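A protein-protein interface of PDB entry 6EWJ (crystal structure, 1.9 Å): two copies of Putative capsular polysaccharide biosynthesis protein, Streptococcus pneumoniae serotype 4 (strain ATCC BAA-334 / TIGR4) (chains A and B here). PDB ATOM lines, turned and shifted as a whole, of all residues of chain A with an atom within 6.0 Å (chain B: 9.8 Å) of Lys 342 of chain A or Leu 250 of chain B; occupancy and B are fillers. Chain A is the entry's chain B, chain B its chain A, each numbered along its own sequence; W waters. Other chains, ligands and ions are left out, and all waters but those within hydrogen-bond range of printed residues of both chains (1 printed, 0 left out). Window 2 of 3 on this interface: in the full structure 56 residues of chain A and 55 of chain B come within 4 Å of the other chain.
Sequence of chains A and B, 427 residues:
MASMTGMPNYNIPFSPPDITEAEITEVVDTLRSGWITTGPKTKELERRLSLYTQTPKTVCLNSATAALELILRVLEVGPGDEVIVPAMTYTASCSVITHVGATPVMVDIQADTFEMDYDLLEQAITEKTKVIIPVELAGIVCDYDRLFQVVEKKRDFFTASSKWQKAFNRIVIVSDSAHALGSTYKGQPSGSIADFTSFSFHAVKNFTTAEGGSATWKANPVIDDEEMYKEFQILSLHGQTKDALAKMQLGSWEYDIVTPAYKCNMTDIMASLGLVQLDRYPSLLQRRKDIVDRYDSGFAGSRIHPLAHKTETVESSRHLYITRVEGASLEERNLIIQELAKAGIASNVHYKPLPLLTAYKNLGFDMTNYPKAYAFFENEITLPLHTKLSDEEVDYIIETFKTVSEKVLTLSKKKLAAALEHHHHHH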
ATOM      1  N   ASN A   9     -22.941 -22.563 -38.066  1.00  0.00           N
ATOM      2  CA  ASN A   9     -23.639 -21.250 -38.058  1.00  0.00           C
ATOM      3  C   ASN A   9     -22.702 -20.089 -37.656  1.00  0.00           C
ATOM      4  O   ASN A   9     -21.519 -20.099 -38.023  1.00  0.00           O
ATOM      5  CB  ASN A   9     -24.899 -21.310 -37.167  1.00  0.00           C
ATOM      6  CG  ASN A   9     -25.886 -20.178 -37.474  1.00  0.00           C
ATOM      7  OD1 ASN A   9     -26.042 -19.779 -38.631  1.00  0.00           O
ATOM      8  ND2 ASN A   9     -26.511 -19.633 -36.441  1.00  0.00           N
ATOM      9  N   LEU A 335     -35.746  -6.213 -27.023  1.00  0.00           N
ATOM     10  CA  LEU A 335     -36.146  -7.353 -27.874  1.00  0.00           C
ATOM     11  C   LEU A 335     -35.156  -7.544 -29.026  1.00  0.00           C
ATOM     12  O   LEU A 335     -34.721  -8.667 -29.279  1.00  0.00           O
ATOM     13  CB  LEU A 335     -37.593  -7.233 -28.386  1.00  0.00           C
ATOM     14  CG  LEU A 335     -38.180  -8.375 -29.256  1.00  0.00           C
ATOM     15  CD1 LEU A 335     -37.959  -9.770 -28.640  1.00  0.00           C
ATOM     16  CD2 LEU A 335     -39.662  -8.169 -29.525  1.00  0.00           C
ATOM     17  N   ILE A 337     -32.007  -6.805 -29.228  1.00  0.00           N
ATOM     18  CA  ILE A 337     -30.767  -7.408 -28.746  1.00  0.00           C
ATOM     19  C   ILE A 337     -30.924  -8.928 -28.547  1.00  0.00           C
ATOM     20  O   ILE A 337     -30.080  -9.700 -28.958  1.00  0.00           O
ATOM     21  CB  ILE A 337     -30.313  -6.760 -27.456  1.00  0.00           C
ATOM     22  CG1 ILE A 337     -29.734  -5.407 -27.774  1.00  0.00           C
ATOM     23  CG2 ILE A 337     -29.284  -7.631 -26.730  1.00  0.00           C
ATOM     24  CD1 ILE A 337     -29.446  -4.601 -26.551  1.00  0.00           C
ATOM     25  N   GLN A 338     -32.009  -9.333 -27.936  1.00  0.00           N
ATOM     26  CA  GLN A 338     -32.270 -10.778 -27.762  1.00  0.00           C
ATOM     27  C   GLN A 338     -32.471 -11.539 -29.097  1.00  0.00           C
ATOM     28  O   GLN A 338     -32.045 -12.696 -29.245  1.00  0.00           O
ATOM     29  CB  GLN A 338     -33.439 -11.020 -26.782  1.00  0.00           C
ATOM     30  CG  GLN A 338     -33.232 -10.420 -25.391  1.00  0.00           C
ATOM     31  CD  GLN A 338     -31.891 -10.822 -24.756  1.00  0.00           C
ATOM     32  OE1 GLN A 338     -31.513 -11.996 -24.802  1.00  0.00           O
ATOM     33  NE2 GLN A 338     -31.215  -9.897 -24.128  1.00  0.00           N
ATOM     34  N   GLU A 339     -33.065 -10.892 -30.081  1.00  0.00           N
ATOM     35  CA  GLU A 339     -33.177 -11.487 -31.421  1.00  0.00           C
ATOM     36  C   GLU A 339     -31.818 -11.580 -32.097  1.00  0.00           C
ATOM     37  O   GLU A 339     -31.592 -12.477 -32.903  1.00  0.00           O
ATOM     38  CB  GLU A 339     -34.114 -10.644 -32.323  1.00  0.00           C
ATOM     39  CG  GLU A 339     -35.575 -10.844 -32.011  1.00  0.00           C
ATOM     40  CD  GLU A 339     -36.086 -12.225 -32.436  1.00  0.00           C
ATOM     41  OE1 GLU A 339     -35.701 -12.707 -33.534  1.00  0.00           O
ATOM     42  OE2 GLU A 339     -36.907 -12.791 -31.710  1.00  0.00           O
ATOM     43  N   LEU A 340     -30.964 -10.559 -31.898  1.00  0.00           N
ATOM     44  CA  LEU A 340     -29.607 -10.606 -32.473  1.00  0.00           C
ATOM     45  C   LEU A 340     -28.866 -11.800 -31.878  1.00  0.00           C
ATOM     46  O   LEU A 340     -28.184 -12.555 -32.576  1.00  0.00           O
ATOM     47  CB  LEU A 340     -28.843  -9.317 -32.215  1.00  0.00           C
ATOM     48  CG  LEU A 340     -29.199  -8.121 -33.096  1.00  0.00           C
ATOM     49  CD1 LEU A 340     -28.531  -6.848 -32.616  1.00  0.00           C
ATOM     50  CD2 LEU A 340     -28.819  -8.418 -34.531  1.00  0.00           C
ATOM     51  N   ALA A 341     -29.086 -11.993 -30.597  1.00  0.00           N
ATOM     52  CA  ALA A 341     -28.457 -13.095 -29.880  1.00  0.00           C
ATOM     53  C   ALA A 341     -28.929 -14.476 -30.381  1.00  0.00           C
ATOM     54  O   ALA A 341     -28.118 -15.368 -30.547  1.00  0.00           O
ATOM     55  CB  ALA A 341     -28.694 -12.945 -28.365  1.00  0.00           C
ATOM     56  N   LYS A 342     -30.220 -14.629 -30.644  1.00  0.00           N
ATOM     57  CA  LYS A 342     -30.744 -15.879 -31.266  1.00  0.00           C
ATOM     58  C   LYS A 342     -30.160 -16.150 -32.655  1.00  0.00           C
ATOM     59  O   LYS A 342     -30.105 -17.290 -33.079  1.00  0.00           O
ATOM     60  CB  LYS A 342     -32.245 -15.866 -31.350  1.00  0.00           C
ATOM     61  CG  LYS A 342     -32.932 -15.975 -30.016  1.00  0.00           C
ATOM     62  CD  LYS A 342     -34.434 -15.971 -30.179  1.00  0.00           C
ATOM     63  CE  LYS A 342     -35.132 -15.668 -28.861  1.00  0.00           C
ATOM     64  NZ  LYS A 342     -36.529 -15.231 -29.137  1.00  0.00           N
ATOM     65  N   ALA A 343     -29.731 -15.080 -33.340  1.00  0.00           N
ATOM     66  CA  ALA A 343     -29.121 -15.167 -34.663  1.00  0.00           C
ATOM     67  C   ALA A 343     -27.604 -15.308 -34.592  1.00  0.00           C
ATOM     68  O   ALA A 343     -26.918 -15.226 -35.602  1.00  0.00           O
ATOM     69  CB  ALA A 343     -29.531 -13.944 -35.499  1.00  0.00           C
ATOM     70  N   GLY A 344     -27.059 -15.503 -33.395  1.00  0.00           N
ATOM     71  CA  GLY A 344     -25.633 -15.698 -33.196  1.00  0.00           C
ATOM     72  C   GLY A 344     -24.793 -14.419 -33.219  1.00  0.00           C
ATOM     73  O   GLY A 344     -23.616 -14.465 -33.584  1.00  0.00           O
ATOM     74  N   ILE A 345     -25.415 -13.292 -32.859  1.00  0.00           N
ATOM     75  CA  ILE A 345     -24.749 -11.981 -32.839  1.00  0.00           C
ATOM     76  C   ILE A 345     -24.816 -11.351 -31.465  1.00  0.00           C
ATOM     77  O   ILE A 345     -25.872 -10.933 -31.016  1.00  0.00           O
ATOM     78  CB  ILE A 345     -25.394 -11.028 -33.849  1.00  0.00           C
ATOM     79  CG1 ILE A 345     -25.307 -11.622 -35.268  1.00  0.00           C
ATOM     80  CG2 ILE A 345     -24.746  -9.672 -33.818  1.00  0.00           C
ATOM     81  CD1 ILE A 345     -26.220 -10.976 -36.248  1.00  0.00           C
ATOM     82  N   ALA B 244     -30.564 -12.541 -11.789  1.00  0.00           N
ATOM     83  CA  ALA B 244     -30.760 -13.889 -12.327  1.00  0.00           C
ATOM     84  C   ALA B 244     -31.301 -13.835 -13.769  1.00  0.00           C
ATOM     85  O   ALA B 244     -30.798 -14.513 -14.648  1.00  0.00           O
ATOM     86  CB  ALA B 244     -31.710 -14.700 -11.448  1.00  0.00           C
ATOM     87  N   LEU B 245     -32.296 -12.995 -13.979  1.00  0.00           N
ATOM     88  CA  LEU B 245     -32.898 -12.794 -15.300  1.00  0.00           C
ATOM     89  C   LEU B 245     -31.863 -12.349 -16.341  1.00  0.00           C
ATOM     90  O   LEU B 245     -31.770 -12.971 -17.391  1.00  0.00           O
ATOM     91  CB  LEU B 245     -34.031 -11.786 -15.217  1.00  0.00           C
ATOM     92  CG  LEU B 245     -34.859 -11.551 -16.475  1.00  0.00           C
ATOM     93  CD1 LEU B 245     -35.640 -12.811 -16.840  1.00  0.00           C
ATOM     94  CD2 LEU B 245     -35.784 -10.381 -16.213  1.00  0.00           C
ATOM     95  N   ALA B 246     -31.037 -11.344 -16.017  1.00  0.00           N
ATOM     96  CA  ALA B 246     -29.987 -10.909 -16.937  1.00  0.00           C
ATOM     97  C   ALA B 246     -28.968 -12.008 -17.310  1.00  0.00           C
ATOM     98  O   ALA B 246     -28.577 -12.138 -18.468  1.00  0.00           O
ATOM     99  CB  ALA B 246     -29.292  -9.675 -16.415  1.00  0.00           C
ATOM    100  N   LYS B 247     -28.596 -12.844 -16.356  1.00  0.00           N
ATOM    101  CA  LYS B 247     -27.643 -13.928 -16.646  1.00  0.00           C
ATOM    102  C   LYS B 247     -28.220 -15.061 -17.479  1.00  0.00           C
ATOM    103  O   LYS B 247     -27.494 -15.711 -18.227  1.00  0.00           O
ATOM    104  CB  LYS B 247     -27.027 -14.508 -15.330  1.00  0.00           C
ATOM    105  CG  LYS B 247     -26.030 -13.578 -14.692  1.00  0.00           C
ATOM    106  CD  LYS B 247     -25.584 -13.920 -13.276  1.00  0.00           C
ATOM    107  CE  LYS B 247     -26.673 -13.809 -12.205  1.00  0.00           C
ATOM    108  NZ  LYS B 247     -26.224 -14.368 -10.868  1.00  0.00           N
ATOM    109  N   MET B 248     -29.506 -15.321 -17.356  1.00  0.00           N
ATOM    110  CA  MET B 248     -30.104 -16.449 -18.064  1.00  0.00           C
ATOM    111  C   MET B 248     -30.372 -16.133 -19.543  1.00  0.00           C
ATOM    112  O   MET B 248     -30.495 -17.036 -20.370  1.00  0.00           O
ATOM    113  CB  MET B 248     -31.400 -16.834 -17.387  1.00  0.00           C
ATOM    114  CG  MET B 248     -32.034 -18.117 -17.927  1.00  0.00           C
ATOM    115  SD  MET B 248     -33.477 -18.586 -16.930  1.00  0.00           S
ATOM    116  CE  MET B 248     -32.602 -19.299 -15.540  1.00  0.00           C
ATOM    117  N   GLN B 249     -30.544 -14.856 -19.832  1.00  0.00           N
ATOM    118  CA  GLN B 249     -30.810 -14.420 -21.180  1.00  0.00           C
ATOM    119  C   GLN B 249     -29.617 -14.715 -22.062  1.00  0.00           C
ATOM    120  O   GLN B 249     -28.491 -14.695 -21.609  1.00  0.00           O
ATOM    121  CB  GLN B 249     -31.188 -12.952 -21.185  1.00  0.00           C
ATOM    122  CG  GLN B 249     -32.626 -12.782 -20.714  1.00  0.00           C
ATOM    123  CD  GLN B 249     -33.035 -11.343 -20.543  1.00  0.00           C
ATOM    124  OE1 GLN B 249     -32.272 -10.527 -19.990  1.00  0.00           O
ATOM    125  NE2 GLN B 249     -34.217 -11.014 -21.008  1.00  0.00           N
ATOM    126  N   LEU B 250     -29.888 -14.990 -23.338  1.00  0.00           N
ATOM    127  CA  LEU B 250     -28.819 -15.249 -24.303  1.00  0.00           C
ATOM    128  C   LEU B 250     -27.905 -14.031 -24.426  1.00  0.00           C
ATOM    129  O   LEU B 250     -26.709 -14.174 -24.527  1.00  0.00           O
ATOM    130  CB  LEU B 250     -29.393 -15.565 -25.687  1.00  0.00           C
ATOM    131  CG  LEU B 250     -29.571 -16.971 -26.186  1.00  0.00           C
ATOM    132  CD1 LEU B 250     -30.033 -16.925 -27.646  1.00  0.00           C
ATOM    133  CD2 LEU B 250     -28.307 -17.822 -26.034  1.00  0.00           C
ATOM    134  N   GLY B 251     -28.514 -12.840 -24.488  1.00  0.00           N
ATOM    135  CA  GLY B 251     -27.779 -11.552 -24.486  1.00  0.00           C
ATOM    136  C   GLY B 251     -27.807 -10.963 -23.104  1.00  0.00           C
ATOM    137  O   GLY B 251     -28.823 -10.407 -22.712  1.00  0.00           O
ATOM    138  N   SER B 252     -26.728 -11.149 -22.329  1.00  0.00           N
ATOM    139  CA  SER B 252     -26.684 -10.786 -20.920  1.00  0.00           C
ATOM    140  C   SER B 252     -25.956  -9.470 -20.708  1.00  0.00           C
ATOM    141  O   SER B 252     -25.026  -9.387 -19.893  1.00  0.00           O
ATOM    142  CB  SER B 252     -25.975 -11.888 -20.080  1.00  0.00           C
ATOM    143  OG  SER B 252     -26.697 -13.075 -20.039  1.00  0.00           O
ATOM    144  N   TRP B 253     -26.399  -8.433 -21.402  1.00  0.00           N
ATOM    145  CA  TRP B 253     -25.729  -7.115 -21.307  1.00  0.00           C
ATOM    146  C   TRP B 253     -26.069  -6.367 -20.010  1.00  0.00           C
ATOM    147  O   TRP B 253     -25.255  -5.662 -19.500  1.00  0.00           O
ATOM    148  CB  TRP B 253     -26.062  -6.248 -22.566  1.00  0.00           C
ATOM    149  CG  TRP B 253     -27.481  -5.866 -22.648  1.00  0.00           C
ATOM    150  CD1 TRP B 253     -28.478  -6.567 -23.250  1.00  0.00           C
ATOM    151  CD2 TRP B 253     -28.088  -4.690 -22.097  1.00  0.00           C
ATOM    152  NE1 TRP B 253     -29.665  -5.932 -23.083  1.00  0.00           N
ATOM    153  CE2 TRP B 253     -29.462  -4.759 -22.406  1.00  0.00           C
ATOM    154  CE3 TRP B 253     -27.607  -3.591 -21.351  1.00  0.00           C
ATOM    155  CZ2 TRP B 253     -30.387  -3.776 -22.001  1.00  0.00           C
ATOM    156  CZ3 TRP B 253     -28.518  -2.605 -20.955  1.00  0.00           C
ATOM    157  CH2 TRP B 253     -29.911  -2.716 -21.294  1.00  0.00           C
ATOM    158  N   GLU B 254     -27.296  -6.498 -19.512  1.00  0.00           N
ATOM    159  CA  GLU B 254     -27.784  -5.578 -18.497  1.00  0.00           C
ATOM    160  C   GLU B 254     -27.176  -5.797 -17.105  1.00  0.00           C
ATOM    161  O   GLU B 254     -27.107  -6.911 -16.624  1.00  0.00           O
ATOM    162  CB  GLU B 254     -29.309  -5.553 -18.464  1.00  0.00           C
ATOM    163  CG  GLU B 254     -29.787  -4.286 -17.832  1.00  0.00           C
ATOM    164  CD  GLU B 254     -31.261  -4.110 -17.829  1.00  0.00           C
ATOM    165  OE1 GLU B 254     -31.967  -4.944 -18.440  1.00  0.00           O
ATOM    166  OE2 GLU B 254     -31.689  -3.123 -17.189  1.00  0.00           O
HETATM  167  O   HOH W   1     -31.846  -7.123 -24.340  1.00  0.00           O
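The side-chain amide nitrogen of Gln 338 of chain A sits at hydrogen-bond distance from the backbone carbonyl oxygen of Gly 251 of chain B, at 2.8 Å.
OG of Ser 252 of chain B lies within hydrogen-bond range of O of Gln 249 of chain B, 2.9 Å away. The side-chain carboxylate (OE2) of Glu 339 of chain A lies within salt-bridge range of the side-chain amino group (NZ) of Lys 342 of chain A.
Among the printed residues, merely in contact across the chains: Ile 337 of chain A with Trp 253 of chain B (3.7 Å), Gln 338 of chain A with Gln 249 of chain B (3.8 Å), Gln 338 of chain A with Leu 250 of chain B (3.7 Å), Ala 341 of chain A with Leu 250 of chain B (3.8 Å), Ala 341 of chain A with Gly 251 of chain B (3.9 Å) and Lys 342 of chain A with Leu 250 of chain B (3.8 Å).
Lys 342 of chain A touches just one residue of chain B: Leu 250. Of chain A, only Gln 338 (3.7 Å), Ala 341 (3.8 Å) and Lys 342 (3.8 Å) come within 4 Å of Leu 250 of chain B. Ala 341 of chain A touches just these residues of chain B: Leu 250 and Gly 251. No residue of chain B comes within 4 Å of Ala 343 of chain A. Of the printed residues of chain A, Trp 253 of chain B touches Ile 337. Of the printed residues of chain B, Gln 338 of chain A touches Gln 249, Leu 250 and Gly 251. Of the printed residues of chain A, Gly 251 of chain B touches Gln 338 (2.8 Å) and Ala 341 (3.9 Å). Of the printed residues of chain B, Ile 337 of chain A touches Trp 253 (3.7 Å). Printed residues of chain A within 4 Å of Gln 249 of chain B: Gln 338. The nearest printed residue of chain A that does not touch Leu 250 of chain B is Ala 343 of chain A (6.0 Å).
Of the 11 printed residues of chain A, 4 touch a printed residue of chain B. Printed residues of chain A that touch a printed residue of chain B: Ile 337, Gln 338, Ala 341 and Lys 342. Of the 11 printed residues of chain B, 4 touch a printed residue of chain A. Hydrophobic or aromatic side chains of chain B that line the printed part of chain A: Leu 250 and Trp 253. Along chain B the printed residues that touch a printed residue of chain A span positions 249 to 253. Among the printed residues, 7 pairs touch across the chains. Among the printed residues, no Asp or Glu carboxylate lies within 4 Å of a Lys or Arg side-chain nitrogen of the other chain.
No position is printed for both chains. Of the 7 pairs that touch across the chains among the printed residues, none has its exchanged pair printed and touching as well.
Water W1 bridges the indole nitrogen of Trp 253 of chain B and the side-chain amide nitrogen of Gln 338 of chain A.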
